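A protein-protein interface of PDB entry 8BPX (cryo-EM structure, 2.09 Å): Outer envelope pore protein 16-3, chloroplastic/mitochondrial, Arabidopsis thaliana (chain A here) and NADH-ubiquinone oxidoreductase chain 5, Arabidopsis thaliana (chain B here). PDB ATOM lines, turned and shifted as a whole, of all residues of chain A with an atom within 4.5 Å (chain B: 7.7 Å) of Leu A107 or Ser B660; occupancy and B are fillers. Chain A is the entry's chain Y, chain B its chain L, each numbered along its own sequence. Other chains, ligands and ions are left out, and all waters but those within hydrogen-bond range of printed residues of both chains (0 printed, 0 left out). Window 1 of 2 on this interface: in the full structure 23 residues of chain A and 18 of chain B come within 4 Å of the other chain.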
ATOM      1  N   PHE A  69     -23.149 -17.104 -24.734  1.00  0.00           N
ATOM      2  CA  PHE A  69     -23.279 -17.505 -26.129  1.00  0.00           C
ATOM      3  C   PHE A  69     -24.719 -17.841 -26.486  1.00  0.00           C
ATOM      4  O   PHE A  69     -25.144 -17.581 -27.615  1.00  0.00           O
ATOM      5  CB  PHE A  69     -22.365 -18.691 -26.435  1.00  0.00           C
ATOM      6  CG  PHE A  69     -20.969 -18.296 -26.824  1.00  0.00           C
ATOM      7  CD1 PHE A  69     -20.472 -17.048 -26.495  1.00  0.00           C
ATOM      8  CD2 PHE A  69     -20.164 -19.165 -27.542  1.00  0.00           C
ATOM      9  CE1 PHE A  69     -19.192 -16.679 -26.854  1.00  0.00           C
ATOM     10  CE2 PHE A  69     -18.882 -18.803 -27.905  1.00  0.00           C
ATOM     11  CZ  PHE A  69     -18.397 -17.554 -27.559  1.00  0.00           C
ATOM     12  N   ILE A  72     -26.309 -14.417 -27.169  1.00  0.00           N
ATOM     13  CA  ILE A  72     -26.019 -13.926 -28.519  1.00  0.00           C
ATOM     14  C   ILE A  72     -26.796 -14.727 -29.560  1.00  0.00           C
ATOM     15  O   ILE A  72     -27.452 -14.160 -30.443  1.00  0.00           O
ATOM     16  CB  ILE A  72     -24.509 -13.937 -28.829  1.00  0.00           C
ATOM     17  CG1 ILE A  72     -23.726 -12.953 -27.957  1.00  0.00           C
ATOM     18  CG2 ILE A  72     -24.266 -13.641 -30.302  1.00  0.00           C
ATOM     19  CD1 ILE A  72     -22.764 -13.597 -26.991  1.00  0.00           C
ATOM     20  N   ALA A 102     -27.333  -7.804 -30.889  1.00  0.00           N
ATOM     21  CA  ALA A 102     -26.806  -8.897 -30.081  1.00  0.00           C
ATOM     22  C   ALA A 102     -25.416  -8.568 -29.558  1.00  0.00           C
ATOM     23  O   ALA A 102     -25.161  -8.640 -28.346  1.00  0.00           O
ATOM     24  CB  ALA A 102     -26.783 -10.187 -30.899  1.00  0.00           C
ATOM     25  N   GLY A 103     -24.508  -8.184 -30.457  1.00  0.00           N
ATOM     26  CA  GLY A 103     -23.155  -7.862 -30.062  1.00  0.00           C
ATOM     27  C   GLY A 103     -23.125  -6.755 -29.036  1.00  0.00           C
ATOM     28  O   GLY A 103     -22.628  -6.955 -27.923  1.00  0.00           O
ATOM     29  N   ALA A 104     -23.698  -5.598 -29.385  1.00  0.00           N
ATOM     30  CA  ALA A 104     -23.742  -4.470 -28.467  1.00  0.00           C
ATOM     31  C   ALA A 104     -24.261  -4.896 -27.102  1.00  0.00           C
ATOM     32  O   ALA A 104     -23.527  -4.860 -26.111  1.00  0.00           O
ATOM     33  CB  ALA A 104     -24.610  -3.353 -29.055  1.00  0.00           C
ATOM     34  N   SER A 105     -25.507  -5.368 -27.049  1.00  0.00           N
ATOM     35  CA  SER A 105     -26.147  -5.675 -25.776  1.00  0.00           C
ATOM     36  C   SER A 105     -25.318  -6.657 -24.958  1.00  0.00           C
ATOM     37  O   SER A 105     -24.835  -6.324 -23.871  1.00  0.00           O
ATOM     38  CB  SER A 105     -27.550  -6.226 -26.025  1.00  0.00           C
ATOM     39  OG  SER A 105     -27.565  -7.060 -27.167  1.00  0.00           O
ATOM     40  N   VAL A 106     -25.129  -7.877 -25.470  1.00  0.00           N
ATOM     41  CA  VAL A 106     -24.543  -8.922 -24.636  1.00  0.00           C
ATOM     42  C   VAL A 106     -23.080  -8.619 -24.330  1.00  0.00           C
ATOM     43  O   VAL A 106     -22.655  -8.650 -23.167  1.00  0.00           O
ATOM     44  CB  VAL A 106     -24.706 -10.298 -25.300  1.00  0.00           C
ATOM     45  CG1 VAL A 106     -23.945 -11.345 -24.509  1.00  0.00           C
ATOM     46  CG2 VAL A 106     -26.173 -10.660 -25.401  1.00  0.00           C
ATOM     47  N   LEU A 107     -22.283  -8.324 -25.362  1.00  0.00           N
ATOM     48  CA  LEU A 107     -20.858  -8.147 -25.138  1.00  0.00           C
ATOM     49  C   LEU A 107     -20.536  -6.850 -24.406  1.00  0.00           C
ATOM     50  O   LEU A 107     -19.460  -6.755 -23.811  1.00  0.00           O
ATOM     51  CB  LEU A 107     -20.111  -8.220 -26.468  1.00  0.00           C
ATOM     52  CG  LEU A 107     -20.331  -9.536 -27.217  1.00  0.00           C
ATOM     53  CD1 LEU A 107     -19.473  -9.612 -28.470  1.00  0.00           C
ATOM     54  CD2 LEU A 107     -20.056 -10.721 -26.310  1.00  0.00           C
ATOM     55  N   GLY A 108     -21.441  -5.870 -24.388  1.00  0.00           N
ATOM     56  CA  GLY A 108     -21.207  -4.681 -23.600  1.00  0.00           C
ATOM     57  C   GLY A 108     -21.705  -4.841 -22.181  1.00  0.00           C
ATOM     58  O   GLY A 108     -21.188  -4.200 -21.263  1.00  0.00           O
ATOM     59  N   TYR A 109     -22.698  -5.716 -21.981  1.00  0.00           N
ATOM     60  CA  TYR A 109     -23.099  -6.088 -20.599  1.00  0.00           C
ATOM     61  C   TYR A 109     -21.930  -6.822 -19.955  1.00  0.00           C
ATOM     62  O   TYR A 109     -21.620  -6.550 -18.800  1.00  0.00           O
ATOM     63  CB  TYR A 109     -24.382  -6.923 -20.522  1.00  0.00           C
ATOM     64  CG  TYR A 109     -24.717  -7.403 -19.136  1.00  0.00           C
ATOM     65  CD1 TYR A 109     -25.455  -6.613 -18.275  1.00  0.00           C
ATOM     66  CD2 TYR A 109     -24.274  -8.631 -18.671  1.00  0.00           C
ATOM     67  CE1 TYR A 109     -25.759  -7.034 -16.994  1.00  0.00           C
ATOM     68  CE2 TYR A 109     -24.568  -9.066 -17.390  1.00  0.00           C
ATOM     69  CZ  TYR A 109     -25.315  -8.263 -16.548  1.00  0.00           C
ATOM     70  OH  TYR A 109     -25.619  -8.670 -15.282  1.00  0.00           O
ATOM     71  N   ARG A 110     -21.317  -7.735 -20.699  1.00  0.00           N
ATOM     72  CA  ARG A 110     -20.195  -8.482 -20.142  1.00  0.00           C
ATOM     73  C   ARG A 110     -18.952  -7.607 -20.015  1.00  0.00           C
ATOM     74  O   ARG A 110     -18.268  -7.629 -18.986  1.00  0.00           O
ATOM     75  CB  ARG A 110     -19.907  -9.713 -21.001  1.00  0.00           C
ATOM     76  CG  ARG A 110     -20.895 -10.850 -20.798  1.00  0.00           C
ATOM     77  CD  ARG A 110     -20.502 -11.719 -19.616  1.00  0.00           C
ATOM     78  NE  ARG A 110     -21.472 -12.778 -19.370  1.00  0.00           N
ATOM     79  CZ  ARG A 110     -22.359 -12.770 -18.384  1.00  0.00           C
ATOM     80  NH1 ARG A 110     -22.422 -11.771 -17.520  1.00  0.00           N
ATOM     81  NH2 ARG A 110     -23.203 -13.788 -18.261  1.00  0.00           N
ATOM     82  N   ALA A 111     -18.642  -6.826 -21.053  1.00  0.00           N
ATOM     83  CA  ALA A 111     -17.445  -5.994 -21.050  1.00  0.00           C
ATOM     84  C   ALA A 111     -17.597  -4.729 -20.217  1.00  0.00           C
ATOM     85  O   ALA A 111     -16.582  -4.127 -19.848  1.00  0.00           O
ATOM     86  CB  ALA A 111     -17.064  -5.617 -22.482  1.00  0.00           C
ATOM     87  N   ALA A 120     -18.203  -4.373 -30.969  1.00  0.00           N
ATOM     88  CA  ALA A 120     -18.734  -5.720 -31.133  1.00  0.00           C
ATOM     89  C   ALA A 120     -19.934  -5.733 -32.067  1.00  0.00           C
ATOM     90  O   ALA A 120     -20.052  -6.620 -32.921  1.00  0.00           O
ATOM     91  CB  ALA A 120     -19.108  -6.301 -29.772  1.00  0.00           C
ATOM     92  N   LEU B 653     -25.065 -18.284 -37.366  1.00  0.00           N
ATOM     93  CA  LEU B 653     -24.801 -18.349 -35.922  1.00  0.00           C
ATOM     94  C   LEU B 653     -23.375 -18.928 -35.737  1.00  0.00           C
ATOM     95  O   LEU B 653     -22.649 -18.323 -34.990  1.00  0.00           O
ATOM     96  CB  LEU B 653     -25.843 -19.207 -35.200  1.00  0.00           C
ATOM     97  CG  LEU B 653     -27.272 -18.659 -35.173  1.00  0.00           C
ATOM     98  CD1 LEU B 653     -28.223 -19.673 -34.558  1.00  0.00           C
ATOM     99  CD2 LEU B 653     -27.328 -17.339 -34.420  1.00  0.00           C
ATOM    100  N   SER B 654     -23.015 -20.003 -36.432  1.00  0.00           N
ATOM    101  CA  SER B 654     -21.632 -20.541 -36.373  1.00  0.00           C
ATOM    102  C   SER B 654     -20.634 -19.388 -36.430  1.00  0.00           C
ATOM    103  O   SER B 654     -19.934 -19.176 -35.425  1.00  0.00           O
ATOM    104  CB  SER B 654     -21.377 -21.560 -37.461  1.00  0.00           C
ATOM    105  OG  SER B 654     -19.985 -21.716 -37.698  1.00  0.00           O
ATOM    106  N   PHE B 655     -20.608 -18.599 -37.501  1.00  0.00           N
ATOM    107  CA  PHE B 655     -19.475 -17.656 -37.664  1.00  0.00           C
ATOM    108  C   PHE B 655     -19.636 -16.473 -36.693  1.00  0.00           C
ATOM    109  O   PHE B 655     -18.610 -15.955 -36.222  1.00  0.00           O
ATOM    110  CB  PHE B 655     -19.342 -17.226 -39.127  1.00  0.00           C
ATOM    111  CG  PHE B 655     -18.591 -18.202 -39.994  1.00  0.00           C
ATOM    112  CD1 PHE B 655     -17.207 -18.247 -39.972  1.00  0.00           C
ATOM    113  CD2 PHE B 655     -19.266 -19.081 -40.823  1.00  0.00           C
ATOM    114  CE1 PHE B 655     -16.515 -19.146 -40.767  1.00  0.00           C
ATOM    115  CE2 PHE B 655     -18.573 -19.981 -41.616  1.00  0.00           C
ATOM    116  CZ  PHE B 655     -17.198 -20.011 -41.587  1.00  0.00           C
ATOM    117  N   ILE B 656     -20.873 -16.083 -36.381  1.00  0.00           N
ATOM    118  CA  ILE B 656     -21.116 -15.032 -35.356  1.00  0.00           C
ATOM    119  C   ILE B 656     -20.504 -15.404 -34.005  1.00  0.00           C
ATOM    120  O   ILE B 656     -19.825 -14.560 -33.401  1.00  0.00           O
ATOM    121  CB  ILE B 656     -22.624 -14.847 -35.211  1.00  0.00           C
ATOM    122  CG1 ILE B 656     -23.290 -14.490 -36.544  1.00  0.00           C
ATOM    123  CG2 ILE B 656     -22.992 -13.822 -34.148  1.00  0.00           C
ATOM    124  CD1 ILE B 656     -22.778 -13.228 -37.188  1.00  0.00           C
ATOM    125  N   LEU B 657     -20.769 -16.628 -33.545  1.00  0.00           N
ATOM    126  CA  LEU B 657     -20.291 -17.013 -32.194  1.00  0.00           C
ATOM    127  C   LEU B 657     -18.750 -17.025 -32.246  1.00  0.00           C
ATOM    128  O   LEU B 657     -18.138 -16.421 -31.371  1.00  0.00           O
ATOM    129  CB  LEU B 657     -21.031 -18.318 -31.857  1.00  0.00           C
ATOM    130  CG  LEU B 657     -22.459 -18.126 -31.366  1.00  0.00           C
ATOM    131  CD1 LEU B 657     -23.125 -19.451 -31.085  1.00  0.00           C
ATOM    132  CD2 LEU B 657     -22.510 -17.224 -30.141  1.00  0.00           C
ATOM    133  N   ILE B 658     -18.169 -17.537 -33.328  1.00  0.00           N
ATOM    134  CA  ILE B 658     -16.684 -17.468 -33.514  1.00  0.00           C
ATOM    135  C   ILE B 658     -16.190 -16.045 -33.247  1.00  0.00           C
ATOM    136  O   ILE B 658     -15.381 -15.863 -32.323  1.00  0.00           O
ATOM    137  CB  ILE B 658     -16.265 -17.929 -34.918  1.00  0.00           C
ATOM    138  CG1 ILE B 658     -16.678 -19.378 -35.184  1.00  0.00           C
ATOM    139  CG2 ILE B 658     -14.772 -17.730 -35.130  1.00  0.00           C
ATOM    140  CD1 ILE B 658     -16.185 -20.356 -34.145  1.00  0.00           C
ATOM    141  N   VAL B 659     -16.615 -15.088 -34.068  1.00  0.00           N
ATOM    142  CA  VAL B 659     -16.126 -13.693 -33.906  1.00  0.00           C
ATOM    143  C   VAL B 659     -16.438 -13.249 -32.478  1.00  0.00           C
ATOM    144  O   VAL B 659     -15.531 -12.725 -31.820  1.00  0.00           O
ATOM    145  CB  VAL B 659     -16.727 -12.746 -34.961  1.00  0.00           C
ATOM    146  CG1 VAL B 659     -16.468 -11.285 -34.630  1.00  0.00           C
ATOM    147  CG2 VAL B 659     -16.226 -13.072 -36.359  1.00  0.00           C
ATOM    148  N   SER B 660     -17.671 -13.459 -32.021  1.00  0.00           N
ATOM    149  CA  SER B 660     -18.051 -12.954 -30.705  1.00  0.00           C
ATOM    150  C   SER B 660     -17.091 -13.418 -29.618  1.00  0.00           C
ATOM    151  O   SER B 660     -16.933 -12.734 -28.602  1.00  0.00           O
ATOM    152  CB  SER B 660     -19.476 -13.385 -30.366  1.00  0.00           C
ATOM    153  OG  SER B 660     -19.747 -13.195 -28.992  1.00  0.00           O
ATOM    154  N   SER B 661     -16.441 -14.570 -29.811  1.00  0.00           N
ATOM    155  CA  SER B 661     -15.509 -15.074 -28.805  1.00  0.00           C
ATOM    156  C   SER B 661     -14.351 -14.112 -28.575  1.00  0.00           C
ATOM    157  O   SER B 661     -13.747 -14.118 -27.497  1.00  0.00           O
ATOM    158  CB  SER B 661     -14.976 -16.444 -29.219  1.00  0.00           C
ATOM    159  OG  SER B 661     -16.033 -17.330 -29.537  1.00  0.00           O
ATOM    160  N   PHE B 662     -14.035 -13.276 -29.564  1.00  0.00           N
ATOM    161  CA  PHE B 662     -12.857 -12.373 -29.457  1.00  0.00           C
ATOM    162  C   PHE B 662     -13.081 -11.397 -28.298  1.00  0.00           C
ATOM    163  O   PHE B 662     -12.106 -11.002 -27.640  1.00  0.00           O
ATOM    164  CB  PHE B 662     -12.605 -11.643 -30.774  1.00  0.00           C
ATOM    165  CG  PHE B 662     -12.310 -12.533 -31.956  1.00  0.00           C
ATOM    166  CD1 PHE B 662     -11.881 -13.839 -31.779  1.00  0.00           C
ATOM    167  CD2 PHE B 662     -12.465 -12.062 -33.250  1.00  0.00           C
ATOM    168  CE1 PHE B 662     -11.618 -14.654 -32.870  1.00  0.00           C
ATOM    169  CE2 PHE B 662     -12.198 -12.877 -34.339  1.00  0.00           C
ATOM    170  CZ  PHE B 662     -11.776 -14.171 -34.147  1.00  0.00           C
ATOM    171  N   TYR B 663     -14.345 -11.047 -28.062  1.00  0.00           N
ATOM    172  CA  TYR B 663     -14.750 -10.044 -27.050  1.00  0.00           C
ATOM    173  C   TYR B 663     -15.171 -10.755 -25.762  1.00  0.00           C
ATOM    174  O   TYR B 663     -16.343 -10.645 -25.353  1.00  0.00           O
ATOM    175  CB  TYR B 663     -15.864  -9.169 -27.621  1.00  0.00           C
ATOM    176  CG  TYR B 663     -15.505  -8.402 -28.866  1.00  0.00           C
ATOM    177  CD1 TYR B 663     -15.755  -8.920 -30.125  1.00  0.00           C
ATOM    178  CD2 TYR B 663     -14.924  -7.149 -28.783  1.00  0.00           C
ATOM    179  CE1 TYR B 663     -15.432  -8.215 -31.271  1.00  0.00           C
ATOM    180  CE2 TYR B 663     -14.593  -6.431 -29.918  1.00  0.00           C
ATOM    181  CZ  TYR B 663     -14.848  -6.965 -31.166  1.00  0.00           C
ATOM    182  OH  TYR B 663     -14.521  -6.258 -32.284  1.00  0.00           O
ATOM    183  N   THR B 664     -14.231 -11.469 -25.146  1.00  0.00           N
ATOM    184  CA  THR B 664     -14.427 -12.206 -23.905  1.00  0.00           C
ATOM    185  C   THR B 664     -13.379 -11.767 -22.894  1.00  0.00           C
ATOM    186  O   THR B 664     -12.186 -11.713 -23.216  1.00  0.00           O
ATOM    187  CB  THR B 664     -14.345 -13.717 -24.144  1.00  0.00           C
ATOM    188  OG1 THR B 664     -15.571 -14.174 -24.728  1.00  0.00           O
ATOM    189  CG2 THR B 664     -14.108 -14.460 -22.837  1.00  0.00           C
ATOM    190  N   LYS B 665     -13.828 -11.449 -21.682  1.00  0.00           N
ATOM    191  CA  LYS B 665     -12.952 -11.001 -20.600  1.00  0.00           C
ATOM    192  C   LYS B 665     -12.149  -9.768 -21.005  1.00  0.00           C
ATOM    193  O   LYS B 665     -12.705  -8.788 -21.497  1.00  0.00           O
ATOM    194  CB  LYS B 665     -12.009 -12.127 -20.165  1.00  0.00           C
ATOM    195  CG  LYS B 665     -12.697 -13.268 -19.438  1.00  0.00           C
ATOM    196  CD  LYS B 665     -11.687 -14.247 -18.860  1.00  0.00           C
ATOM    197  CE  LYS B 665     -11.490 -14.023 -17.369  1.00  0.00           C
ATOM    198  NZ  LYS B 665     -10.684 -12.802 -17.096  1.00  0.00           N
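The side-chain hydroxyl of Ser B661 lies close to the backbone carbonyl oxygen of Ile B658 (3.2 Å). The backbone carbonyl oxygen (O) of Leu B657 lies within hydrogen-bond range of the side-chain hydroxyl (OG) of Ser B661 (2.9 Å). O of Ser B661 sits at hydrogen-bond distance from OG1 of Thr B664 (3.3 Å).
Among the printed residues, pairs that only touch across the chains: Phe A69 with Leu B657 (3.7 Å), Phe A69 with Ser B661 (3.1 Å), Ile A72 with Leu B657 (3.99 Å), Ile A72 with Ser B660 (3.6 Å), Leu A107 with Ser B660 (3.6 Å) and Leu A107 with Tyr B663 (3.7 Å).
Printed residues of chain B within 4 Å of Ile A72: Leu B657 and Ser B660. Tyr A109 touches none of the printed residues of chain B. Printed residues of chain A within 4 Å of Leu B657: Phe A69 and Ile A72. Ser B660 touches just these residues of chain A: Ile A72 (3.6 Å) and Leu A107 (3.6 Å). Of the printed residues of chain A, Ser B661 touches Phe A69 (3.1 Å).
Of the 13 printed residues of chain B, 4 touch a printed residue of chain A. Along chain B the printed residues that touch a printed residue of chain A span positions 657 to 663. Of the 13 printed residues of chain A, 3 touch a printed residue of chain B. Printed residues of chain A that touch a printed residue of chain B: Phe A69, Ile A72 and Leu A107. Hydrophobic or aromatic side chains of chain A that line the printed part of chain B: Phe A69, Ile A72 and Leu A107. Along chain A the printed residues that touch a printed residue of chain B span positions 69 to 107.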
